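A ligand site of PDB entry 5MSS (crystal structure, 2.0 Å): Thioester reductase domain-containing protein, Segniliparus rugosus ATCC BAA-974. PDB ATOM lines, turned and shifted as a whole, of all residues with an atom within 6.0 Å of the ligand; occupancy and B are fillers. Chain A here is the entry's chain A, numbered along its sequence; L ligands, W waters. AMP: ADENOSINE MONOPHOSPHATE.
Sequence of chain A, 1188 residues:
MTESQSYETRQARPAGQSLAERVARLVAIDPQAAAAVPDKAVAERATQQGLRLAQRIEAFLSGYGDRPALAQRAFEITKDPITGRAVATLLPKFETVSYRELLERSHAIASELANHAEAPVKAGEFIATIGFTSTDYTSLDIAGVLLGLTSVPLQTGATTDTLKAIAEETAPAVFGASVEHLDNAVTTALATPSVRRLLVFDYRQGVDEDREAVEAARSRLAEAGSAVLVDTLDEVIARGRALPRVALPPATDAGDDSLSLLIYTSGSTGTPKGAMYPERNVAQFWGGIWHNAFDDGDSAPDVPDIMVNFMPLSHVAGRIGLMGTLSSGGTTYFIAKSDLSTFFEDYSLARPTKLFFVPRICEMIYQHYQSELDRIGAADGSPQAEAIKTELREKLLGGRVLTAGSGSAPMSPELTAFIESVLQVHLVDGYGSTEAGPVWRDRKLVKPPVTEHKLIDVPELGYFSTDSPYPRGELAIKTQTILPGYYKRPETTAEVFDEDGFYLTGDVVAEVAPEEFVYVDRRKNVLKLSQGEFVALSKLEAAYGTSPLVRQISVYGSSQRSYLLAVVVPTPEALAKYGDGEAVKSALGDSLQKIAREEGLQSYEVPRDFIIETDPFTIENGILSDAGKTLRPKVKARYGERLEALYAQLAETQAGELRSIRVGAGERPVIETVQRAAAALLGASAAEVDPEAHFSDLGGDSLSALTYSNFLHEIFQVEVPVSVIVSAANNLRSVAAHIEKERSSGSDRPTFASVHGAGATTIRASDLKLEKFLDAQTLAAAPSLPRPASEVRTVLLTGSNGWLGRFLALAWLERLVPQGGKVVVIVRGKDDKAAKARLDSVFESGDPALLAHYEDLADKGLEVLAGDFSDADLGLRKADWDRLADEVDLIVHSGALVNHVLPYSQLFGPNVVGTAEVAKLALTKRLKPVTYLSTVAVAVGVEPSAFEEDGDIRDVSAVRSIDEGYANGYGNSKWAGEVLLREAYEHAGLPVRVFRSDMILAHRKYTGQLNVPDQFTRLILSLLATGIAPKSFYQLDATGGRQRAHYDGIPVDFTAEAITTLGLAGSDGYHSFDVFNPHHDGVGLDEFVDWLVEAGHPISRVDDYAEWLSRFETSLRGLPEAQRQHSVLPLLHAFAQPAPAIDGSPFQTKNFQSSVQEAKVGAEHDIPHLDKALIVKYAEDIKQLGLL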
ATOM      1  N   THR A 265      30.308 -34.557  -7.258  1.00  0.00           N
ATOM      2  CA  THR A 265      30.889 -34.024  -8.472  1.00  0.00           C
ATOM      3  C   THR A 265      32.421 -34.171  -8.422  1.00  0.00           C
ATOM      4  O   THR A 265      33.051 -34.098  -7.393  1.00  0.00           O
ATOM      5  CB  THR A 265      30.430 -32.512  -8.716  1.00  0.00           C
ATOM      6  OG1 THR A 265      31.237 -31.841  -9.711  1.00  0.00           O
ATOM      7  CG2 THR A 265      30.542 -31.726  -7.448  1.00  0.00           C
ATOM      8  N   HIS A 315      22.380 -36.447 -11.758  1.00  0.00           N
ATOM      9  CA  HIS A 315      23.064 -35.361 -12.488  1.00  0.00           C
ATOM     10  C   HIS A 315      22.163 -34.159 -12.223  1.00  0.00           C
ATOM     11  O   HIS A 315      20.983 -34.286 -12.289  1.00  0.00           O
ATOM     12  CB  HIS A 315      23.128 -35.745 -13.981  1.00  0.00           C
ATOM     13  CG  HIS A 315      23.997 -34.843 -14.819  1.00  0.00           C
ATOM     14  ND1 HIS A 315      23.684 -33.519 -15.082  1.00  0.00           N
ATOM     15  CD2 HIS A 315      25.138 -35.096 -15.504  1.00  0.00           C
ATOM     16  CE1 HIS A 315      24.612 -32.982 -15.849  1.00  0.00           C
ATOM     17  NE2 HIS A 315      25.518 -33.917 -16.128  1.00  0.00           N
ATOM     18  N   VAL A 316      22.713 -33.044 -11.800  1.00  0.00           N
ATOM     19  CA  VAL A 316      21.905 -31.829 -11.526  1.00  0.00           C
ATOM     20  C   VAL A 316      20.947 -31.481 -12.668  1.00  0.00           C
ATOM     21  O   VAL A 316      19.832 -31.059 -12.390  1.00  0.00           O
ATOM     22  CB  VAL A 316      22.750 -30.609 -11.095  1.00  0.00           C
ATOM     23  CG1 VAL A 316      23.410 -29.894 -12.253  1.00  0.00           C
ATOM     24  CG2 VAL A 316      21.896 -29.622 -10.322  1.00  0.00           C
ATOM     25  N   ALA A 317      21.322 -31.744 -13.905  1.00  0.00           N
ATOM     26  CA  ALA A 317      20.429 -31.534 -15.023  1.00  0.00           C
ATOM     27  C   ALA A 317      19.185 -32.456 -15.021  1.00  0.00           C
ATOM     28  O   ALA A 317      18.161 -32.083 -15.551  1.00  0.00           O
ATOM     29  CB  ALA A 317      21.157 -31.658 -16.348  1.00  0.00           C
ATOM     30  N   SER A 406      20.019 -26.017 -24.376  1.00  0.00           N
ATOM     31  CA  SER A 406      21.035 -26.922 -23.963  1.00  0.00           C
ATOM     32  C   SER A 406      22.038 -26.334 -22.958  1.00  0.00           C
ATOM     33  O   SER A 406      22.122 -25.158 -22.739  1.00  0.00           O
ATOM     34  CB  SER A 406      21.786 -27.553 -25.144  1.00  0.00           C
ATOM     35  OG  SER A 406      22.544 -26.550 -25.719  1.00  0.00           O
ATOM     36  N   GLY A 407      22.831 -27.204 -22.410  1.00  0.00           N
ATOM     37  CA  GLY A 407      23.775 -26.846 -21.357  1.00  0.00           C
ATOM     38  C   GLY A 407      24.509 -28.093 -20.907  1.00  0.00           C
ATOM     39  O   GLY A 407      24.422 -29.144 -21.540  1.00  0.00           O
ATOM     40  N   SER A 408      25.364 -27.935 -19.890  1.00  0.00           N
ATOM     41  CA  SER A 408      26.292 -28.974 -19.392  1.00  0.00           C
ATOM     42  C   SER A 408      27.597 -29.021 -20.073  1.00  0.00           C
ATOM     43  O   SER A 408      28.514 -29.553 -19.526  1.00  0.00           O
ATOM     44  CB  SER A 408      25.703 -30.376 -19.414  1.00  0.00           C
ATOM     45  OG  SER A 408      24.577 -30.341 -18.612  1.00  0.00           O
ATOM     46  N   ALA A 409      27.679 -28.471 -21.285  1.00  0.00           N
ATOM     47  CA  ALA A 409      28.900 -28.458 -22.062  1.00  0.00           C
ATOM     48  C   ALA A 409      28.680 -27.492 -23.192  1.00  0.00           C
ATOM     49  O   ALA A 409      27.579 -27.178 -23.465  1.00  0.00           O
ATOM     50  CB  ALA A 409      29.235 -29.883 -22.610  1.00  0.00           C
ATOM     51  N   PRO A 410      29.744 -26.950 -23.775  1.00  0.00           N
ATOM     52  CA  PRO A 410      29.561 -25.964 -24.860  1.00  0.00           C
ATOM     53  C   PRO A 410      29.126 -26.605 -26.165  1.00  0.00           C
ATOM     54  O   PRO A 410      29.283 -27.839 -26.408  1.00  0.00           O
ATOM     55  CB  PRO A 410      30.958 -25.346 -25.052  1.00  0.00           C
ATOM     56  CG  PRO A 410      31.866 -26.556 -24.713  1.00  0.00           C
ATOM     57  CD  PRO A 410      31.174 -27.161 -23.469  1.00  0.00           C
ATOM     58  N   MET A 411      28.536 -25.801 -27.015  1.00  0.00           N
ATOM     59  CA  MET A 411      28.117 -26.253 -28.323  1.00  0.00           C
ATOM     60  C   MET A 411      28.751 -25.393 -29.403  1.00  0.00           C
ATOM     61  O   MET A 411      28.749 -24.167 -29.289  1.00  0.00           O
ATOM     62  CB  MET A 411      26.614 -26.154 -28.454  1.00  0.00           C
ATOM     63  CG  MET A 411      26.099 -27.084 -29.564  1.00  0.00           C
ATOM     64  SD  MET A 411      24.650 -28.000 -29.106  1.00  0.00           S
ATOM     65  CE  MET A 411      23.618 -26.616 -28.699  1.00  0.00           C
ATOM     66  N   ASP A 429      21.130 -21.167 -24.496  1.00  0.00           N
ATOM     67  CA  ASP A 429      22.323 -21.798 -23.856  1.00  0.00           C
ATOM     68  C   ASP A 429      22.335 -21.433 -22.400  1.00  0.00           C
ATOM     69  O   ASP A 429      22.352 -20.291 -22.075  1.00  0.00           O
ATOM     70  CB  ASP A 429      23.653 -21.372 -24.500  1.00  0.00           C
ATOM     71  CG  ASP A 429      24.835 -21.645 -23.606  1.00  0.00           C
ATOM     72  OD1 ASP A 429      25.038 -22.824 -23.314  1.00  0.00           O
ATOM     73  OD2 ASP A 429      25.641 -20.741 -23.283  1.00  0.00           O
ATOM     74  N   GLY A 430      22.275 -22.449 -21.537  1.00  0.00           N
ATOM     75  CA  GLY A 430      22.267 -22.275 -20.107  1.00  0.00           C
ATOM     76  C   GLY A 430      23.512 -22.785 -19.497  1.00  0.00           C
ATOM     77  O   GLY A 430      23.784 -24.008 -19.601  1.00  0.00           O
ATOM     78  N   TYR A 431      24.266 -21.886 -18.876  1.00  0.00           N
ATOM     79  CA  TYR A 431      25.523 -22.204 -18.108  1.00  0.00           C
ATOM     80  C   TYR A 431      25.257 -22.084 -16.588  1.00  0.00           C
ATOM     81  O   TYR A 431      24.701 -21.130 -16.118  1.00  0.00           O
ATOM     82  CB  TYR A 431      26.651 -21.256 -18.529  1.00  0.00           C
ATOM     83  CG  TYR A 431      27.861 -21.312 -17.652  1.00  0.00           C
ATOM     84  CD1 TYR A 431      28.823 -22.317 -17.774  1.00  0.00           C
ATOM     85  CD2 TYR A 431      28.021 -20.401 -16.655  1.00  0.00           C
ATOM     86  CE1 TYR A 431      29.877 -22.405 -16.883  1.00  0.00           C
ATOM     87  CE2 TYR A 431      29.062 -20.447 -15.789  1.00  0.00           C
ATOM     88  CZ  TYR A 431      29.974 -21.453 -15.879  1.00  0.00           C
ATOM     89  OH  TYR A 431      31.008 -21.447 -14.961  1.00  0.00           O
ATOM     90  N   GLY A 432      25.654 -23.098 -15.839  1.00  0.00           N
ATOM     91  CA  GLY A 432      25.746 -23.068 -14.426  1.00  0.00           C
ATOM     92  C   GLY A 432      26.371 -24.334 -13.943  1.00  0.00           C
ATOM     93  O   GLY A 432      26.979 -25.064 -14.778  1.00  0.00           O
ATOM     94  N   SER A 433      26.301 -24.583 -12.634  1.00  0.00           N
ATOM     95  CA  SER A 433      26.958 -25.714 -12.042  1.00  0.00           C
ATOM     96  C   SER A 433      26.242 -26.164 -10.765  1.00  0.00           C
ATOM     97  O   SER A 433      25.509 -25.431 -10.116  1.00  0.00           O
ATOM     98  CB  SER A 433      28.408 -25.362 -11.723  1.00  0.00           C
ATOM     99  OG  SER A 433      28.513 -24.293 -10.811  1.00  0.00           O
ATOM    100  N   THR A 434      26.631 -27.344 -10.367  1.00  0.00           N
ATOM    101  CA  THR A 434      26.264 -27.934  -9.107  1.00  0.00           C
ATOM    102  C   THR A 434      26.606 -27.020  -7.935  1.00  0.00           C
ATOM    103  O   THR A 434      25.771 -26.828  -7.045  1.00  0.00           O
ATOM    104  CB  THR A 434      27.011 -29.275  -8.954  1.00  0.00           C
ATOM    105  OG1 THR A 434      26.497 -30.210  -9.906  1.00  0.00           O
ATOM    106  CG2 THR A 434      26.826 -29.825  -7.625  1.00  0.00           C
ATOM    107  N   GLU A 435      27.785 -26.442  -7.941  1.00  0.00           N
ATOM    108  CA  GLU A 435      28.229 -25.581  -6.890  1.00  0.00           C
ATOM    109  C   GLU A 435      27.556 -24.178  -6.880  1.00  0.00           C
ATOM    110  O   GLU A 435      27.236 -23.700  -5.867  1.00  0.00           O
ATOM    111  CB  GLU A 435      29.699 -25.381  -7.019  1.00  0.00           C
ATOM    112  CG  GLU A 435      30.598 -26.525  -6.632  1.00  0.00           C
ATOM    113  CD  GLU A 435      30.942 -27.483  -7.762  1.00  0.00           C
ATOM    114  OE1 GLU A 435      30.335 -27.413  -8.883  1.00  0.00           O
ATOM    115  OE2 GLU A 435      31.808 -28.321  -7.535  1.00  0.00           O
ATOM    116  N   TRP A 440      24.646 -18.149 -16.271  1.00  0.00           N
ATOM    117  CA  TRP A 440      24.287 -17.312 -17.443  1.00  0.00           C
ATOM    118  C   TRP A 440      23.270 -17.990 -18.363  1.00  0.00           C
ATOM    119  O   TRP A 440      23.147 -19.236 -18.439  1.00  0.00           O
ATOM    120  CB  TRP A 440      25.545 -16.798 -18.249  1.00  0.00           C
ATOM    121  CG  TRP A 440      26.214 -17.670 -19.226  1.00  0.00           C
ATOM    122  CD1 TRP A 440      25.629 -18.252 -20.331  1.00  0.00           C
ATOM    123  CD2 TRP A 440      27.611 -17.961 -19.320  1.00  0.00           C
ATOM    124  NE1 TRP A 440      26.559 -18.969 -21.005  1.00  0.00           N
ATOM    125  CE2 TRP A 440      27.787 -18.783 -20.441  1.00  0.00           C
ATOM    126  CE3 TRP A 440      28.718 -17.635 -18.534  1.00  0.00           C
ATOM    127  CZ2 TRP A 440      29.016 -19.283 -20.827  1.00  0.00           C
ATOM    128  CZ3 TRP A 440      29.966 -18.123 -18.916  1.00  0.00           C
ATOM    129  CH2 TRP A 440      30.113 -18.928 -20.062  1.00  0.00           C
ATOM    130  N   THR A 505      35.049 -20.744 -10.424  1.00  0.00           N
ATOM    131  CA  THR A 505      34.319 -21.763 -11.238  1.00  0.00           C
ATOM    132  C   THR A 505      35.274 -22.859 -11.840  1.00  0.00           C
ATOM    133  O   THR A 505      34.813 -23.905 -12.210  1.00  0.00           O
ATOM    134  CB  THR A 505      33.570 -21.078 -12.440  1.00  0.00           C
ATOM    135  OG1 THR A 505      34.549 -20.427 -13.337  1.00  0.00           O
ATOM    136  CG2 THR A 505      32.569 -20.093 -11.907  1.00  0.00           C
ATOM    137  N   ASP A 507      36.436 -22.378 -14.749  1.00  0.00           N
ATOM    138  CA  ASP A 507      36.087 -22.212 -16.141  1.00  0.00           C
ATOM    139  C   ASP A 507      36.693 -20.907 -16.662  1.00  0.00           C
ATOM    140  O   ASP A 507      36.419 -19.849 -16.151  1.00  0.00           O
ATOM    141  CB  ASP A 507      34.564 -22.186 -16.380  1.00  0.00           C
ATOM    142  CG  ASP A 507      33.831 -23.459 -16.022  1.00  0.00           C
ATOM    143  OD1 ASP A 507      34.355 -24.577 -16.394  1.00  0.00           O
ATOM    144  OD2 ASP A 507      32.739 -23.374 -15.328  1.00  0.00           O
ATOM    145  N   TYR A 519      32.321 -19.355 -23.048  1.00  0.00           N
ATOM    146  CA  TYR A 519      33.144 -20.434 -22.493  1.00  0.00           C
ATOM    147  C   TYR A 519      34.365 -20.699 -23.397  1.00  0.00           C
ATOM    148  O   TYR A 519      34.207 -20.866 -24.596  1.00  0.00           O
ATOM    149  CB  TYR A 519      32.316 -21.734 -22.292  1.00  0.00           C
ATOM    150  CG  TYR A 519      33.121 -22.869 -21.735  1.00  0.00           C
ATOM    151  CD1 TYR A 519      33.836 -23.754 -22.608  1.00  0.00           C
ATOM    152  CD2 TYR A 519      33.291 -23.031 -20.389  1.00  0.00           C
ATOM    153  CE1 TYR A 519      34.620 -24.739 -22.089  1.00  0.00           C
ATOM    154  CE2 TYR A 519      34.031 -24.025 -19.895  1.00  0.00           C
ATOM    155  CZ  TYR A 519      34.675 -24.909 -20.744  1.00  0.00           C
ATOM    156  OH  TYR A 519      35.447 -25.914 -20.286  1.00  0.00           O
ATOM    157  N   ARG A 522      39.325 -24.675 -19.382  1.00  0.00           N
ATOM    158  CA  ARG A 522      39.416 -24.929 -17.968  1.00  0.00           C
ATOM    159  C   ARG A 522      40.780 -24.483 -17.448  1.00  0.00           C
ATOM    160  O   ARG A 522      41.778 -24.572 -18.172  1.00  0.00           O
ATOM    161  CB  ARG A 522      39.191 -26.405 -17.663  1.00  0.00           C
ATOM    162  CG  ARG A 522      37.697 -26.820 -17.890  1.00  0.00           C
ATOM    163  CD  ARG A 522      37.201 -27.593 -16.655  1.00  0.00           C
ATOM    164  NE  ARG A 522      36.437 -26.791 -15.829  1.00  0.00           N
ATOM    165  CZ  ARG A 522      36.123 -26.940 -14.532  1.00  0.00           C
ATOM    166  NH1 ARG A 522      36.494 -27.920 -13.698  1.00  0.00           N
ATOM    167  NH2 ARG A 522      35.386 -25.977 -14.091  1.00  0.00           N
ATOM    168  N   LYS A 528      34.521 -31.208 -19.173  1.00  0.00           N
ATOM    169  CA  LYS A 528      33.261 -31.792 -19.718  1.00  0.00           C
ATOM    170  C   LYS A 528      33.527 -32.179 -21.128  1.00  0.00           C
ATOM    171  O   LYS A 528      34.305 -31.484 -21.819  1.00  0.00           O
ATOM    172  CB  LYS A 528      32.171 -30.730 -19.755  1.00  0.00           C
ATOM    173  CG  LYS A 528      31.462 -30.328 -18.415  1.00  0.00           C
ATOM    174  CD  LYS A 528      30.891 -31.527 -17.632  1.00  0.00           C
ATOM    175  CE  LYS A 528      30.211 -31.143 -16.321  1.00  0.00           C
ATOM    176  NZ  LYS A 528      28.845 -30.752 -16.619  1.00  0.00           N
ATOM    177  N   GLY A 532      28.115 -34.072 -21.239  1.00  0.00           N
ATOM    178  CA  GLY A 532      27.853 -33.322 -20.051  1.00  0.00           C
ATOM    179  C   GLY A 532      28.454 -33.862 -18.769  1.00  0.00           C
ATOM    180  O   GLY A 532      28.043 -33.372 -17.731  1.00  0.00           O
ATOM    181  N   PHE A 534      32.000 -34.802 -16.319  1.00  0.00           N
ATOM    182  CA  PHE A 534      33.378 -34.373 -16.226  1.00  0.00           C
ATOM    183  C   PHE A 534      34.227 -35.610 -16.473  1.00  0.00           C
ATOM    184  O   PHE A 534      33.828 -36.705 -16.060  1.00  0.00           O
ATOM    185  CB  PHE A 534      33.670 -33.883 -14.806  1.00  0.00           C
ATOM    186  CG  PHE A 534      33.321 -32.441 -14.547  1.00  0.00           C
ATOM    187  CD1 PHE A 534      33.950 -31.439 -15.245  1.00  0.00           C
ATOM    188  CD2 PHE A 534      32.448 -32.093 -13.536  1.00  0.00           C
ATOM    189  CE1 PHE A 534      33.668 -30.116 -15.025  1.00  0.00           C
ATOM    190  CE2 PHE A 534      32.161 -30.713 -13.272  1.00  0.00           C
ATOM    191  CZ  PHE A 534      32.787 -29.752 -14.031  1.00  0.00           C
HETATM  192  P   AMP L   1      27.798 -29.632 -13.313  1.00  0.00           P
HETATM  193  O1P AMP L   1      26.522 -28.853 -13.628  1.00  0.00           O
HETATM  194  O2P AMP L   1      27.576 -31.050 -13.758  1.00  0.00           O
HETATM  195  O3P AMP L   1      28.372 -29.228 -11.991  1.00  0.00           O
HETATM  196  O5' AMP L   1      28.910 -29.109 -14.350  1.00  0.00           O
HETATM  197  C5' AMP L   1      29.169 -27.737 -14.521  1.00  0.00           C
HETATM  198  C4' AMP L   1      30.311 -27.539 -15.507  1.00  0.00           C
HETATM  199  O4' AMP L   1      29.815 -27.912 -16.825  1.00  0.00           O
HETATM  200  C3' AMP L   1      30.717 -26.058 -15.582  1.00  0.00           C
HETATM  201  O3' AMP L   1      31.672 -25.562 -14.603  1.00  0.00           O
HETATM  202  C2' AMP L   1      31.224 -25.983 -17.005  1.00  0.00           C
HETATM  203  O2' AMP L   1      32.541 -26.460 -17.066  1.00  0.00           O
HETATM  204  C1' AMP L   1      30.308 -26.935 -17.750  1.00  0.00           C
HETATM  205  N9  AMP L   1      29.163 -26.256 -18.358  1.00  0.00           N
HETATM  206  C8  AMP L   1      27.872 -26.251 -17.880  1.00  0.00           C
HETATM  207  N7  AMP L   1      27.072 -25.564 -18.738  1.00  0.00           N
HETATM  208  C5  AMP L   1      27.816 -25.159 -19.730  1.00  0.00           C
HETATM  209  C6  AMP L   1      27.573 -24.362 -20.911  1.00  0.00           C
HETATM  210  N6  AMP L   1      26.329 -23.964 -21.164  1.00  0.00           N
HETATM  211  N1  AMP L   1      28.652 -24.098 -21.709  1.00  0.00           N
HETATM  212  C2  AMP L   1      29.878 -24.536 -21.428  1.00  0.00           C
HETATM  213  N3  AMP L   1      30.158 -25.300 -20.367  1.00  0.00           N
HETATM  214  C4  AMP L   1      29.185 -25.622 -19.502  1.00  0.00           C
HETATM  215  O   HOH W   1      25.554 -32.691 -11.519  1.00  0.00           O
HETATM  216  O   HOH W   2      28.157 -22.193 -23.515  1.00  0.00           O
HETATM  217  O   HOH W   3      31.992 -26.956 -12.221  1.00  0.00           O
HETATM  218  O   HOH W   4      34.198 -28.259 -19.008  1.00  0.00           O
HETATM  219  O   HOH W   5      32.103 -24.403 -11.417  1.00  0.00           O
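Merely in contact with the ligand: Val 316 (3.6 Å), Gly 407 (3.9 Å), Ala 409 (3.6 Å), Pro 410 (3.4 Å), Tyr 431 (3.6 Å), Gly 432 (3.4 Å), Ser 433 (3.5 Å), Tyr 519 (3.7 Å), Arg 522 (3.8 Å) and Phe 534 (3.6 Å). Within 4 Å of the ligand: Val 316, Gly 407, Ser 408, Ala 409, Pro 410, Asp 429, Gly 430, Tyr 431, Gly 432, Ser 433, Thr 434, Asp 507, Tyr 519, Arg 522, Lys 528 and Phe 534. Along chain A the residues within 4 Å of the ligand span positions 316 to 534.
O3' of the ligand sits at hydrogen-bond distance from OD2 of Asp 507 (2.5 Å). A nitrogen (N6) of the ligand lies within hydrogen-bond range of the side-chain carboxylate (OD1) of Asp 429 (2.8 Å). The side-chain amino group (NZ) of Lys 528 is in salt-bridge range of an oxygen (O2P) of the ligand (3.1 Å). An oxygen (O3P) of the ligand sits at hydrogen-bond distance from the backbone NH (N) of Thr 434. The side-chain hydroxyl of Thr 434 sits at hydrogen-bond distance from an oxygen (O3P) of the ligand (3.0 Å). A nitrogen (N6) of the ligand sits at hydrogen-bond distance from the backbone carbonyl oxygen of Gly 430, at 3.0 Å. A nitrogen (N7) of the ligand sits at hydrogen-bond distance from the backbone NH (N) of Ser 408 (3.1 Å).
Water W2 lies within hydrogen-bond range of N1 of the ligand (2.7 Å) and OD2 of Asp 429 (2.9 Å). Water W4 lies within hydrogen-bond range of the side-chain hydroxyl of Tyr 519, the backbone NH of Lys 528 and an oxygen (O2') of the ligand. Water W5 lies within hydrogen-bond range of O of Thr 505 (2.9 Å) and O3' of the ligand (3.4 Å). Water W1 lies within hydrogen-bond range of the backbone NH (N) of Val 316 (2.9 Å), the side-chain hydroxyl (OG1) of Thr 434 (3.1 Å) and an oxygen (O2P) of the ligand (3.4 Å).
OH of Tyr 431 sits at hydrogen-bond distance from OD2 of Asp 507. The guanidinium group (NH2) of Arg 522 is in salt-bridge range of the side-chain carboxylate (OD1) of Asp 507 (2.9 Å). The side-chain carboxylate of Asp 429 lies within hydrogen-bond range of the indole nitrogen of Trp 440, 3.0 Å away. NZ of Lys 528 lies within hydrogen-bond range of O of Ser 408, at 3.2 Å. NZ of Lys 528 lies within hydrogen-bond range of O of Gly 532 (3.0 Å). O of Ser 406 lies within hydrogen-bond range of N of Gly 430 (3.0 Å). The backbone carbonyl oxygen of Trp 440 lies within hydrogen-bond range of the backbone NH of Tyr 431. NH2 of Arg 522 is in hydrogen-bond range of O of Thr 505 (2.9 Å).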
